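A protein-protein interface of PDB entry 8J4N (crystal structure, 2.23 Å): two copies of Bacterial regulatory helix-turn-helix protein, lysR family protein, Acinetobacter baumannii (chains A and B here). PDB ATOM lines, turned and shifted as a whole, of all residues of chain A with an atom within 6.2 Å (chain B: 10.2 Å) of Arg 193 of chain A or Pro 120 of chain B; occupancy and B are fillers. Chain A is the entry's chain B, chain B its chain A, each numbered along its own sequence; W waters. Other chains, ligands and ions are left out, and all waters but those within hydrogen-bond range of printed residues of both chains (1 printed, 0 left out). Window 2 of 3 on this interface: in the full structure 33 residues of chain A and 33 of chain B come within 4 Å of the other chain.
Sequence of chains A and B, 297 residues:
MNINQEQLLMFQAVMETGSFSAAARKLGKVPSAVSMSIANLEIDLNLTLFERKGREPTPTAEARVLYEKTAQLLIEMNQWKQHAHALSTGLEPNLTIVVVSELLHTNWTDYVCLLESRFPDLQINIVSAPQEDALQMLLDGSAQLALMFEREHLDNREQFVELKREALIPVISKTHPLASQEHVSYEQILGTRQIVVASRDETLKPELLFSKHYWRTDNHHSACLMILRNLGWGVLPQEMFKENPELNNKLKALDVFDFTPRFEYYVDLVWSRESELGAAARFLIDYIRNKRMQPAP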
ATOM      1  N   HIS A 176     -20.076  18.051  -9.888  1.00  0.00           N
ATOM      2  CA  HIS A 176     -20.037  16.859 -10.721  1.00  0.00           C
ATOM      3  C   HIS A 176     -20.436  17.224 -12.152  1.00  0.00           C
ATOM      4  O   HIS A 176     -21.338  18.042 -12.348  1.00  0.00           O
ATOM      5  CB  HIS A 176     -20.978  15.789 -10.157  1.00  0.00           C
ATOM      6  CG  HIS A 176     -20.771  14.424 -10.741  1.00  0.00           C
ATOM      7  ND1 HIS A 176     -21.192  14.082 -12.009  1.00  0.00           N
ATOM      8  CD2 HIS A 176     -20.202  13.311 -10.223  1.00  0.00           C
ATOM      9  CE1 HIS A 176     -20.885  12.821 -12.249  1.00  0.00           C
ATOM     10  NE2 HIS A 176     -20.282  12.329 -11.182  1.00  0.00           N
ATOM     11  N   ILE A 189     -27.786   8.244 -15.713  1.00  0.00           N
ATOM     12  CA  ILE A 189     -27.742   7.632 -14.386  1.00  0.00           C
ATOM     13  C   ILE A 189     -27.139   6.234 -14.468  1.00  0.00           C
ATOM     14  O   ILE A 189     -26.330   5.833 -13.625  1.00  0.00           O
ATOM     15  CB  ILE A 189     -29.147   7.602 -13.758  1.00  0.00           C
ATOM     16  CG1 ILE A 189     -29.688   9.019 -13.582  1.00  0.00           C
ATOM     17  CG2 ILE A 189     -29.116   6.881 -12.420  1.00  0.00           C
ATOM     18  CD1 ILE A 189     -28.744   9.940 -12.815  1.00  0.00           C
ATOM     19  N   LEU A 190     -27.533   5.472 -15.491  1.00  0.00           N
ATOM     20  CA  LEU A 190     -26.985   4.133 -15.696  1.00  0.00           C
ATOM     21  C   LEU A 190     -25.463   4.152 -15.763  1.00  0.00           C
ATOM     22  O   LEU A 190     -24.798   3.252 -15.234  1.00  0.00           O
ATOM     23  CB  LEU A 190     -27.566   3.527 -16.976  1.00  0.00           C
ATOM     24  CG  LEU A 190     -27.406   2.022 -17.190  1.00  0.00           C
ATOM     25  CD1 LEU A 190     -28.158   1.244 -16.129  1.00  0.00           C
ATOM     26  CD2 LEU A 190     -27.884   1.626 -18.572  1.00  0.00           C
ATOM     27  N   GLY A 191     -24.896   5.171 -16.398  1.00  0.00           N
ATOM     28  CA  GLY A 191     -23.466   5.306 -16.555  1.00  0.00           C
ATOM     29  C   GLY A 191     -22.760   6.094 -15.474  1.00  0.00           C
ATOM     30  O   GLY A 191     -21.567   6.385 -15.613  1.00  0.00           O
ATOM     31  N   THR A 192     -23.452   6.460 -14.402  1.00  0.00           N
ATOM     32  CA  THR A 192     -22.855   7.185 -13.290  1.00  0.00           C
ATOM     33  C   THR A 192     -22.791   6.271 -12.076  1.00  0.00           C
ATOM     34  O   THR A 192     -23.706   5.478 -11.844  1.00  0.00           O
ATOM     35  CB  THR A 192     -23.656   8.450 -12.959  1.00  0.00           C
ATOM     36  OG1 THR A 192     -23.928   9.177 -14.165  1.00  0.00           O
ATOM     37  CG2 THR A 192     -22.880   9.340 -12.003  1.00  0.00           C
ATOM     38  N   ARG A 193     -21.704   6.367 -11.313  1.00  0.00           N
ATOM     39  CA  ARG A 193     -21.560   5.541 -10.121  1.00  0.00           C
ATOM     40  C   ARG A 193     -22.574   5.950  -9.057  1.00  0.00           C
ATOM     41  O   ARG A 193     -22.717   7.135  -8.741  1.00  0.00           O
ATOM     42  CB  ARG A 193     -20.146   5.650  -9.556  1.00  0.00           C
ATOM     43  CG  ARG A 193     -19.919   4.743  -8.355  1.00  0.00           C
ATOM     44  CD  ARG A 193     -18.589   5.002  -7.678  1.00  0.00           C
ATOM     45  NE  ARG A 193     -17.459   4.617  -8.513  1.00  0.00           N
ATOM     46  CZ  ARG A 193     -16.528   5.458  -8.942  1.00  0.00           C
ATOM     47  NH1 ARG A 193     -16.577   6.750  -8.657  1.00  0.00           N
ATOM     48  NH2 ARG A 193     -15.525   4.993  -9.681  1.00  0.00           N
ATOM     49  N   GLN A 194     -23.279   4.963  -8.507  1.00  0.00           N
ATOM     50  CA  GLN A 194     -24.224   5.184  -7.421  1.00  0.00           C
ATOM     51  C   GLN A 194     -23.586   4.784  -6.098  1.00  0.00           C
ATOM     52  O   GLN A 194     -22.962   3.723  -6.001  1.00  0.00           O
ATOM     53  CB  GLN A 194     -25.510   4.386  -7.641  1.00  0.00           C
ATOM     54  CG  GLN A 194     -26.569   4.624  -6.573  1.00  0.00           C
ATOM     55  CD  GLN A 194     -27.841   3.842  -6.820  1.00  0.00           C
ATOM     56  OE1 GLN A 194     -27.985   3.175  -7.846  1.00  0.00           O
ATOM     57  NE2 GLN A 194     -28.773   3.916  -5.874  1.00  0.00           N
ATOM     58  N   ILE A 195     -23.737   5.633  -5.087  1.00  0.00           N
ATOM     59  CA  ILE A 195     -23.311   5.311  -3.731  1.00  0.00           C
ATOM     60  C   ILE A 195     -24.538   4.807  -2.983  1.00  0.00           C
ATOM     61  O   ILE A 195     -25.486   5.562  -2.746  1.00  0.00           O
ATOM     62  CB  ILE A 195     -22.687   6.522  -3.031  1.00  0.00           C
ATOM     63  CG1 ILE A 195     -21.621   7.159  -3.923  1.00  0.00           C
ATOM     64  CG2 ILE A 195     -22.082   6.110  -1.706  1.00  0.00           C
ATOM     65  CD1 ILE A 195     -20.510   6.208  -4.306  1.00  0.00           C
ATOM     66  N   SER A 211     -27.906   2.257 -11.275  1.00  0.00           N
ATOM     67  CA  SER A 211     -26.669   2.440 -12.009  1.00  0.00           C
ATOM     68  C   SER A 211     -25.998   1.090 -12.203  1.00  0.00           C
ATOM     69  O   SER A 211     -26.127   0.187 -11.370  1.00  0.00           O
ATOM     70  CB  SER A 211     -25.733   3.392 -11.271  1.00  0.00           C
ATOM     71  OG  SER A 211     -26.332   4.666 -11.107  1.00  0.00           O
ATOM     72  N   HIS A 213     -22.738   0.537 -12.204  1.00  0.00           N
ATOM     73  CA  HIS A 213     -21.628   0.443 -11.267  1.00  0.00           C
ATOM     74  C   HIS A 213     -21.959   1.219 -10.000  1.00  0.00           C
ATOM     75  O   HIS A 213     -22.508   2.323 -10.060  1.00  0.00           O
ATOM     76  CB  HIS A 213     -20.339   0.970 -11.898  1.00  0.00           C
ATOM     77  CG  HIS A 213     -19.883   0.169 -13.077  1.00  0.00           C
ATOM     78  ND1 HIS A 213     -19.582  -1.175 -12.992  1.00  0.00           N
ATOM     79  CD2 HIS A 213     -19.695   0.513 -14.373  1.00  0.00           C
ATOM     80  CE1 HIS A 213     -19.219  -1.620 -14.182  1.00  0.00           C
ATOM     81  NE2 HIS A 213     -19.280  -0.616 -15.037  1.00  0.00           N
ATOM     82  N   TYR A 214     -21.619   0.638  -8.852  1.00  0.00           N
ATOM     83  CA  TYR A 214     -22.047   1.191  -7.578  1.00  0.00           C
ATOM     84  C   TYR A 214     -21.078   0.782  -6.481  1.00  0.00           C
ATOM     85  O   TYR A 214     -20.401  -0.247  -6.574  1.00  0.00           O
ATOM     86  CB  TYR A 214     -23.473   0.736  -7.231  1.00  0.00           C
ATOM     87  CG  TYR A 214     -23.605  -0.741  -6.911  1.00  0.00           C
ATOM     88  CD1 TYR A 214     -23.348  -1.225  -5.633  1.00  0.00           C
ATOM     89  CD2 TYR A 214     -23.982  -1.654  -7.889  1.00  0.00           C
ATOM     90  CE1 TYR A 214     -23.460  -2.569  -5.340  1.00  0.00           C
ATOM     91  CE2 TYR A 214     -24.107  -3.002  -7.601  1.00  0.00           C
ATOM     92  CZ  TYR A 214     -23.844  -3.453  -6.326  1.00  0.00           C
ATOM     93  OH  TYR A 214     -23.963  -4.795  -6.039  1.00  0.00           O
ATOM     94  N   TRP A 215     -21.027   1.608  -5.440  1.00  0.00           N
ATOM     95  CA  TRP A 215     -20.355   1.297  -4.190  1.00  0.00           C
ATOM     96  C   TRP A 215     -21.395   1.129  -3.092  1.00  0.00           C
ATOM     97  O   TRP A 215     -22.436   1.792  -3.093  1.00  0.00           O
ATOM     98  CB  TRP A 215     -19.381   2.404  -3.786  1.00  0.00           C
ATOM     99  CG  TRP A 215     -18.171   2.531  -4.641  1.00  0.00           C
ATOM    100  CD1 TRP A 215     -17.843   1.776  -5.728  1.00  0.00           C
ATOM    101  CD2 TRP A 215     -17.123   3.488  -4.484  1.00  0.00           C
ATOM    102  NE1 TRP A 215     -16.648   2.203  -6.254  1.00  0.00           N
ATOM    103  CE2 TRP A 215     -16.186   3.255  -5.507  1.00  0.00           C
ATOM    104  CE3 TRP A 215     -16.885   4.520  -3.572  1.00  0.00           C
ATOM    105  CZ2 TRP A 215     -15.028   4.017  -5.646  1.00  0.00           C
ATOM    106  CZ3 TRP A 215     -15.738   5.274  -3.710  1.00  0.00           C
ATOM    107  CH2 TRP A 215     -14.824   5.019  -4.737  1.00  0.00           C
ATOM    108  N   ASN A 230     -17.353  13.983  -5.218  1.00  0.00           N
ATOM    109  CA  ASN A 230     -17.690  13.750  -6.625  1.00  0.00           C
ATOM    110  C   ASN A 230     -17.502  12.293  -7.034  1.00  0.00           C
ATOM    111  O   ASN A 230     -17.277  11.999  -8.209  1.00  0.00           O
ATOM    112  CB  ASN A 230     -16.887  14.658  -7.563  1.00  0.00           C
ATOM    113  CG  ASN A 230     -17.274  16.114  -7.434  1.00  0.00           C
ATOM    114  OD1 ASN A 230     -17.925  16.507  -6.471  1.00  0.00           O
ATOM    115  ND2 ASN A 230     -16.888  16.922  -8.415  1.00  0.00           N
ATOM    116  N   LEU A 231     -17.581  11.367  -6.084  1.00  0.00           N
ATOM    117  CA  LEU A 231     -17.408   9.961  -6.423  1.00  0.00           C
ATOM    118  C   LEU A 231     -18.683   9.321  -6.962  1.00  0.00           C
ATOM    119  O   LEU A 231     -18.625   8.181  -7.438  1.00  0.00           O
ATOM    120  CB  LEU A 231     -16.899   9.188  -5.204  1.00  0.00           C
ATOM    121  CG  LEU A 231     -15.490   9.592  -4.765  1.00  0.00           C
ATOM    122  CD1 LEU A 231     -15.144   9.012  -3.398  1.00  0.00           C
ATOM    123  CD2 LEU A 231     -14.459   9.187  -5.812  1.00  0.00           C
ATOM    124  N   GLY A 232     -19.811  10.018  -6.913  1.00  0.00           N
ATOM    125  CA  GLY A 232     -21.038   9.492  -7.475  1.00  0.00           C
ATOM    126  C   GLY A 232     -22.249  10.222  -6.935  1.00  0.00           C
ATOM    127  O   GLY A 232     -22.141  11.276  -6.307  1.00  0.00           O
ATOM    128  N   TRP A 233     -23.411   9.635  -7.208  1.00  0.00           N
ATOM    129  CA  TRP A 233     -24.686  10.135  -6.726  1.00  0.00           C
ATOM    130  C   TRP A 233     -25.285   9.145  -5.738  1.00  0.00           C
ATOM    131  O   TRP A 233     -24.876   7.983  -5.662  1.00  0.00           O
ATOM    132  CB  TRP A 233     -25.662  10.377  -7.880  1.00  0.00           C
ATOM    133  CG  TRP A 233     -26.241   9.117  -8.451  1.00  0.00           C
ATOM    134  CD1 TRP A 233     -25.648   8.269  -9.341  1.00  0.00           C
ATOM    135  CD2 TRP A 233     -27.528   8.557  -8.161  1.00  0.00           C
ATOM    136  NE1 TRP A 233     -26.489   7.221  -9.628  1.00  0.00           N
ATOM    137  CE2 TRP A 233     -27.649   7.373  -8.915  1.00  0.00           C
ATOM    138  CE3 TRP A 233     -28.591   8.942  -7.337  1.00  0.00           C
ATOM    139  CZ2 TRP A 233     -28.787   6.572  -8.873  1.00  0.00           C
ATOM    140  CZ3 TRP A 233     -29.722   8.143  -7.297  1.00  0.00           C
ATOM    141  CH2 TRP A 233     -29.811   6.974  -8.061  1.00  0.00           C
ATOM    142  N   GLY A 234     -26.269   9.621  -4.984  1.00  0.00           N
ATOM    143  CA  GLY A 234     -26.882   8.782  -3.973  1.00  0.00           C
ATOM    144  C   GLY A 234     -28.118   9.433  -3.397  1.00  0.00           C
ATOM    145  O   GLY A 234     -28.508  10.538  -3.786  1.00  0.00           O
ATOM    146  N   GLU B  92     -15.330  -8.838 -11.318  1.00  0.00           N
ATOM    147  CA  GLU B  92     -15.601  -7.521 -10.738  1.00  0.00           C
ATOM    148  C   GLU B  92     -14.796  -7.369  -9.451  1.00  0.00           C
ATOM    149  O   GLU B  92     -15.136  -7.978  -8.426  1.00  0.00           O
ATOM    150  CB  GLU B  92     -17.102  -7.312 -10.492  1.00  0.00           C
ATOM    151  CG  GLU B  92     -17.502  -6.125  -9.621  1.00  0.00           C
ATOM    152  CD  GLU B  92     -17.179  -4.758 -10.202  1.00  0.00           C
ATOM    153  OE1 GLU B  92     -16.471  -4.650 -11.224  1.00  0.00           O
ATOM    154  OE2 GLU B  92     -17.645  -3.764  -9.613  1.00  0.00           O
ATOM    155  N   PRO B  93     -13.722  -6.575  -9.460  1.00  0.00           N
ATOM    156  CA  PRO B  93     -12.854  -6.493  -8.278  1.00  0.00           C
ATOM    157  C   PRO B  93     -13.478  -5.671  -7.160  1.00  0.00           C
ATOM    158  O   PRO B  93     -14.136  -4.653  -7.394  1.00  0.00           O
ATOM    159  CB  PRO B  93     -11.578  -5.836  -8.814  1.00  0.00           C
ATOM    160  CG  PRO B  93     -11.990  -5.092 -10.030  1.00  0.00           C
ATOM    161  CD  PRO B  93     -13.273  -5.693 -10.555  1.00  0.00           C
ATOM    162  N   VAL B 112      -9.809   6.979   0.113  1.00  0.00           N
ATOM    163  CA  VAL B 112     -10.746   6.440  -0.866  1.00  0.00           C
ATOM    164  C   VAL B 112     -10.551   7.116  -2.219  1.00  0.00           C
ATOM    165  O   VAL B 112     -10.514   6.454  -3.261  1.00  0.00           O
ATOM    166  CB  VAL B 112     -12.191   6.589  -0.359  1.00  0.00           C
ATOM    167  CG1 VAL B 112     -13.177   6.094  -1.404  1.00  0.00           C
ATOM    168  CG2 VAL B 112     -12.368   5.825   0.944  1.00  0.00           C
ATOM    169  N   CYS B 113     -10.419   8.446  -2.223  1.00  0.00           N
ATOM    170  CA  CYS B 113     -10.191   9.163  -3.477  1.00  0.00           C
ATOM    171  C   CYS B 113      -8.875   8.744  -4.124  1.00  0.00           C
ATOM    172  O   CYS B 113      -8.779   8.646  -5.354  1.00  0.00           O
ATOM    173  CB  CYS B 113     -10.211  10.673  -3.229  1.00  0.00           C
ATOM    174  SG  CYS B 113     -11.802  11.310  -2.652  1.00  0.00           S
ATOM    175  N   LEU B 114      -7.848   8.492  -3.311  1.00  0.00           N
ATOM    176  CA  LEU B 114      -6.577   8.003  -3.839  1.00  0.00           C
ATOM    177  C   LEU B 114      -6.754   6.655  -4.528  1.00  0.00           C
ATOM    178  O   LEU B 114      -6.232   6.428  -5.627  1.00  0.00           O
ATOM    179  CB  LEU B 114      -5.552   7.895  -2.710  1.00  0.00           C
ATOM    180  CG  LEU B 114      -4.185   7.314  -3.078  1.00  0.00           C
ATOM    181  CD1 LEU B 114      -3.467   8.223  -4.069  1.00  0.00           C
ATOM    182  CD2 LEU B 114      -3.347   7.085  -1.829  1.00  0.00           C
ATOM    183  N   LEU B 115      -7.497   5.748  -3.889  1.00  0.00           N
ATOM    184  CA  LEU B 115      -7.725   4.428  -4.466  1.00  0.00           C
ATOM    185  C   LEU B 115      -8.579   4.513  -5.724  1.00  0.00           C
ATOM    186  O   LEU B 115      -8.325   3.801  -6.703  1.00  0.00           O
ATOM    187  CB  LEU B 115      -8.385   3.522  -3.430  1.00  0.00           C
ATOM    188  CG  LEU B 115      -7.457   2.982  -2.340  1.00  0.00           C
ATOM    189  CD1 LEU B 115      -8.223   2.103  -1.384  1.00  0.00           C
ATOM    190  CD2 LEU B 115      -6.296   2.208  -2.942  1.00  0.00           C
ATOM    191  N   GLU B 116      -9.594   5.379  -5.718  1.00  0.00           N
ATOM    192  CA  GLU B 116     -10.492   5.474  -6.865  1.00  0.00           C
ATOM    193  C   GLU B 116      -9.775   6.020  -8.093  1.00  0.00           C
ATOM    194  O   GLU B 116      -9.975   5.524  -9.207  1.00  0.00           O
ATOM    195  CB  GLU B 116     -11.699   6.348  -6.518  1.00  0.00           C
ATOM    196  CG  GLU B 116     -12.823   6.305  -7.549  1.00  0.00           C
ATOM    197  CD  GLU B 116     -12.627   7.296  -8.683  1.00  0.00           C
ATOM    198  OE1 GLU B 116     -11.832   8.244  -8.519  1.00  0.00           O
ATOM    199  OE2 GLU B 116     -13.271   7.129  -9.740  1.00  0.00           O
ATOM    200  N   SER B 117      -8.940   7.043  -7.911  1.00  0.00           N
ATOM    201  CA  SER B 117      -8.234   7.635  -9.044  1.00  0.00           C
ATOM    202  C   SER B 117      -7.209   6.677  -9.640  1.00  0.00           C
ATOM    203  O   SER B 117      -6.901   6.764 -10.834  1.00  0.00           O
ATOM    204  CB  SER B 117      -7.552   8.933  -8.613  1.00  0.00           C
ATOM    205  OG  SER B 117      -6.517   8.668  -7.680  1.00  0.00           O
ATOM    206  N   ARG B 118      -6.667   5.772  -8.829  1.00  0.00           N
ATOM    207  CA  ARG B 118      -5.682   4.800  -9.289  1.00  0.00           C
ATOM    208  C   ARG B 118      -6.329   3.522  -9.811  1.00  0.00           C
ATOM    209  O   ARG B 118      -5.798   2.898 -10.737  1.00  0.00           O
ATOM    210  CB  ARG B 118      -4.718   4.467  -8.145  1.00  0.00           C
ATOM    211  CG  ARG B 118      -3.678   3.389  -8.426  1.00  0.00           C
ATOM    212  CD  ARG B 118      -2.560   3.834  -9.362  1.00  0.00           C
ATOM    213  NE  ARG B 118      -1.589   2.759  -9.534  1.00  0.00           N
ATOM    214  CZ  ARG B 118      -1.822   1.642 -10.208  1.00  0.00           C
ATOM    215  NH1 ARG B 118      -2.920   1.486 -10.929  1.00  0.00           N
ATOM    216  NH2 ARG B 118      -0.927   0.658 -10.163  1.00  0.00           N
ATOM    217  N   PHE B 119      -7.469   3.127  -9.251  1.00  0.00           N
ATOM    218  CA  PHE B 119      -8.174   1.905  -9.638  1.00  0.00           C
ATOM    219  C   PHE B 119      -9.603   2.256  -9.993  1.00  0.00           C
ATOM    220  O   PHE B 119     -10.539   2.022  -9.211  1.00  0.00           O
ATOM    221  CB  PHE B 119      -8.131   0.881  -8.510  1.00  0.00           C
ATOM    222  CG  PHE B 119      -6.725   0.459  -8.131  1.00  0.00           C
ATOM    223  CD1 PHE B 119      -6.069  -0.527  -8.846  1.00  0.00           C
ATOM    224  CD2 PHE B 119      -6.063   1.037  -7.050  1.00  0.00           C
ATOM    225  CE1 PHE B 119      -4.791  -0.926  -8.512  1.00  0.00           C
ATOM    226  CE2 PHE B 119      -4.784   0.645  -6.706  1.00  0.00           C
ATOM    227  CZ  PHE B 119      -4.144  -0.336  -7.437  1.00  0.00           C
ATOM    228  N   PRO B 120      -9.829   2.841 -11.173  1.00  0.00           N
ATOM    229  CA  PRO B 120     -11.159   3.418 -11.456  1.00  0.00           C
ATOM    230  C   PRO B 120     -12.272   2.388 -11.607  1.00  0.00           C
ATOM    231  O   PRO B 120     -13.450   2.750 -11.480  1.00  0.00           O
ATOM    232  CB  PRO B 120     -10.966   4.205 -12.772  1.00  0.00           C
ATOM    233  CG  PRO B 120      -9.669   3.759 -13.336  1.00  0.00           C
ATOM    234  CD  PRO B 120      -8.923   2.921 -12.340  1.00  0.00           C
ATOM    235  N   ASP B 121     -11.951   1.126 -11.868  1.00  0.00           N
ATOM    236  CA  ASP B 121     -12.970   0.091 -11.995  1.00  0.00           C
ATOM    237  C   ASP B 121     -13.207  -0.667 -10.697  1.00  0.00           C
ATOM    238  O   ASP B 121     -13.980  -1.631 -10.691  1.00  0.00           O
ATOM    239  CB  ASP B 121     -12.580  -0.891 -13.100  1.00  0.00           C
ATOM    240  CG  ASP B 121     -12.362  -0.207 -14.426  1.00  0.00           C
ATOM    241  OD1 ASP B 121     -13.178   0.666 -14.791  1.00  0.00           O
ATOM    242  OD2 ASP B 121     -11.362  -0.526 -15.101  1.00  0.00           O
ATOM    243  N   LEU B 122     -12.570  -0.253  -9.608  1.00  0.00           N
ATOM    244  CA  LEU B 122     -12.643  -0.981  -8.349  1.00  0.00           C
ATOM    245  C   LEU B 122     -13.897  -0.601  -7.572  1.00  0.00           C
ATOM    246  O   LEU B 122     -14.165   0.584  -7.352  1.00  0.00           O
ATOM    247  CB  LEU B 122     -11.402  -0.690  -7.509  1.00  0.00           C
ATOM    248  CG  LEU B 122     -11.272  -1.420  -6.172  1.00  0.00           C
ATOM    249  CD1 LEU B 122     -10.965  -2.898  -6.363  1.00  0.00           C
ATOM    250  CD2 LEU B 122     -10.228  -0.741  -5.310  1.00  0.00           C
ATOM    251  N   GLN B 123     -14.666  -1.605  -7.150  1.00  0.00           N
ATOM    252  CA  GLN B 123     -15.744  -1.366  -6.198  1.00  0.00           C
ATOM    253  C   GLN B 123     -15.145  -1.250  -4.804  1.00  0.00           C
ATOM    254  O   GLN B 123     -14.445  -2.161  -4.344  1.00  0.00           O
ATOM    255  CB  GLN B 123     -16.794  -2.474  -6.233  1.00  0.00           C
ATOM    256  CG  GLN B 123     -17.908  -2.226  -5.224  1.00  0.00           C
ATOM    257  CD  GLN B 123     -18.949  -3.325  -5.183  1.00  0.00           C
ATOM    258  OE1 GLN B 123     -18.677  -4.438  -4.743  1.00  0.00           O
ATOM    259  NE2 GLN B 123     -20.160  -3.006  -5.622  1.00  0.00           N
ATOM    260  N   ILE B 124     -15.414  -0.134  -4.137  1.00  0.00           N
ATOM    261  CA  ILE B 124     -14.875   0.152  -2.814  1.00  0.00           C
ATOM    262  C   ILE B 124     -16.052   0.263  -1.856  1.00  0.00           C
ATOM    263  O   ILE B 124     -16.842   1.210  -1.943  1.00  0.00           O
ATOM    264  CB  ILE B 124     -14.035   1.432  -2.806  1.00  0.00           C
ATOM    265  CG1 ILE B 124     -12.806   1.260  -3.700  1.00  0.00           C
ATOM    266  CG2 ILE B 124     -13.625   1.779  -1.387  1.00  0.00           C
ATOM    267  CD1 ILE B 124     -12.111   2.555  -4.027  1.00  0.00           C
ATOM    268  N   ASN B 125     -16.171  -0.700  -0.946  1.00  0.00           N
ATOM    269  CA  ASN B 125     -17.238  -0.710   0.044  1.00  0.00           C
ATOM    270  C   ASN B 125     -16.689  -0.301   1.403  1.00  0.00           C
ATOM    271  O   ASN B 125     -15.753  -0.922   1.916  1.00  0.00           O
ATOM    272  CB  ASN B 125     -17.897  -2.088   0.125  1.00  0.00           C
ATOM    273  CG  ASN B 125     -18.317  -2.609  -1.238  1.00  0.00           C
ATOM    274  OD1 ASN B 125     -19.054  -1.943  -1.968  1.00  0.00           O
ATOM    275  ND2 ASN B 125     -17.857  -3.804  -1.586  1.00  0.00           N
ATOM    276  N   ALA B 280      -5.125  -3.287  -4.798  1.00  0.00           N
ATOM    277  CA  ALA B 280      -5.517  -1.983  -4.271  1.00  0.00           C
ATOM    278  C   ALA B 280      -5.045  -1.798  -2.834  1.00  0.00           C
ATOM    279  O   ALA B 280      -4.479  -0.757  -2.484  1.00  0.00           O
ATOM    280  CB  ALA B 280      -7.033  -1.818  -4.361  1.00  0.00           C
ATOM    281  N   PHE B 283      -1.299  -1.325  -2.737  1.00  0.00           N
ATOM    282  CA  PHE B 283      -0.921   0.012  -3.182  1.00  0.00           C
ATOM    283  C   PHE B 283      -1.039   1.018  -2.044  1.00  0.00           C
ATOM    284  O   PHE B 283      -0.124   1.817  -1.807  1.00  0.00           O
ATOM    285  CB  PHE B 283      -1.792   0.436  -4.364  1.00  0.00           C
ATOM    286  CG  PHE B 283      -1.620   1.877  -4.753  1.00  0.00           C
ATOM    287  CD1 PHE B 283      -0.583   2.263  -5.586  1.00  0.00           C
ATOM    288  CD2 PHE B 283      -2.485   2.849  -4.271  1.00  0.00           C
ATOM    289  CE1 PHE B 283      -0.416   3.588  -5.940  1.00  0.00           C
ATOM    290  CE2 PHE B 283      -2.322   4.176  -4.618  1.00  0.00           C
ATOM    291  CZ  PHE B 283      -1.287   4.544  -5.454  1.00  0.00           C
HETATM  292  O   HOH W   1     -20.560  -2.519  -9.175  1.00  0.00           O
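O of Leu 122 of chain B is in hydrogen-bond range of NE1 of Trp 215 of chain A, at 3.2 Å. The side-chain amide nitrogen of Gln 123 of chain B lies within hydrogen-bond range of the backbone carbonyl oxygen of Tyr 214 of chain A, 2.9 Å away. OE2 of Glu 116 of chain B lies within salt-bridge range of NH2 of Arg 193 of chain A. NE1 of Trp 215 of chain A lies close to N of Ile 124 of chain B (3.4 Å).
O of Arg 193 of chain A sits at hydrogen-bond distance from N of Trp 233 of chain A (3.0 Å). The backbone NH of Trp 215 of chain A sits at hydrogen-bond distance from the backbone carbonyl oxygen of Gln 194 of chain A, 2.9 Å away. O of Pro 93 of chain B lies within hydrogen-bond range of N of Gln 123 of chain B, at 3.1 Å. The backbone carbonyl oxygen (O) of Leu 231 of chain A is in hydrogen-bond range of the guanidinium group (NH1) of Arg 193 of chain A, 2.8 Å away. The side-chain amide oxygen (OE1) of Gln 123 of chain B lies within hydrogen-bond range of the side-chain amide nitrogen (ND2) of Asn 125 of chain B (3.3 Å).
Among the printed residues, merely in contact across the chains: Arg 193 of chain A with Pro 120 of chain B (3.5 Å), Trp 215 of chain A with Val 112 of chain B (3.5 Å), Trp 215 of chain A with Glu 116 of chain B (3.7 Å), Trp 215 of chain A with Gln 123 of chain B (3.7 Å) and Leu 231 of chain A with Glu 116 of chain B (3.7 Å).
Of chain B, only Glu 116 (3.1 Å) and Pro 120 (3.5 Å) come within 4 Å of Arg 193 of chain A. Of chain A, only Arg 193 comes within 4 Å of Pro 120 of chain B. Gly 191 of chain A touches none of the printed residues of chain B. No residue of chain B comes within 4 Å of Thr 192 of chain A. Leu 231 of chain A touches one residue of chain B. No residue of chain B comes within 4 Å of Gly 232 of chain A. Of the printed residues of chain B, Trp 215 of chain A touches Val 112 (3.5 Å), Glu 116 (3.7 Å), Leu 122 (3.2 Å), Gln 123 (3.7 Å) and Ile 124 (3.3 Å). Of the printed residues of chain A, Gln 123 of chain B touches Tyr 214 (2.9 Å) and Trp 215 (3.7 Å). His 176 of chain A touches none of the printed residues of chain B. The nearest printed residue of chain A that does not touch Pro 120 of chain B is Trp 215 of chain A (6.2 Å). The nearest printed residue of chain A that does not touch Leu 122 of chain B is Arg 193 of chain A (5.2 Å).
Of the 18 printed residues of chain B, 6 touch a printed residue of chain A. Hydrophobic or aromatic side chains of chain B that line the printed part of chain A: Val 112 and Ile 124. Among the printed residues, Asp or Glu carboxylates within 4 Å of a Lys or Arg side-chain nitrogen of the other chain: Arg 193 of chain A with Glu 116 of chain B (3.1 Å).
No position is printed for both chains. Of the 9 pairs that touch across the chains among the printed residues, none has its exchanged pair printed and touching as well.
Water W1 lies within hydrogen-bond range of the side-chain carboxylate of Glu 92 of chain B (3.2 Å) and the backbone NH of Tyr 214 of chain A (3.3 Å).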
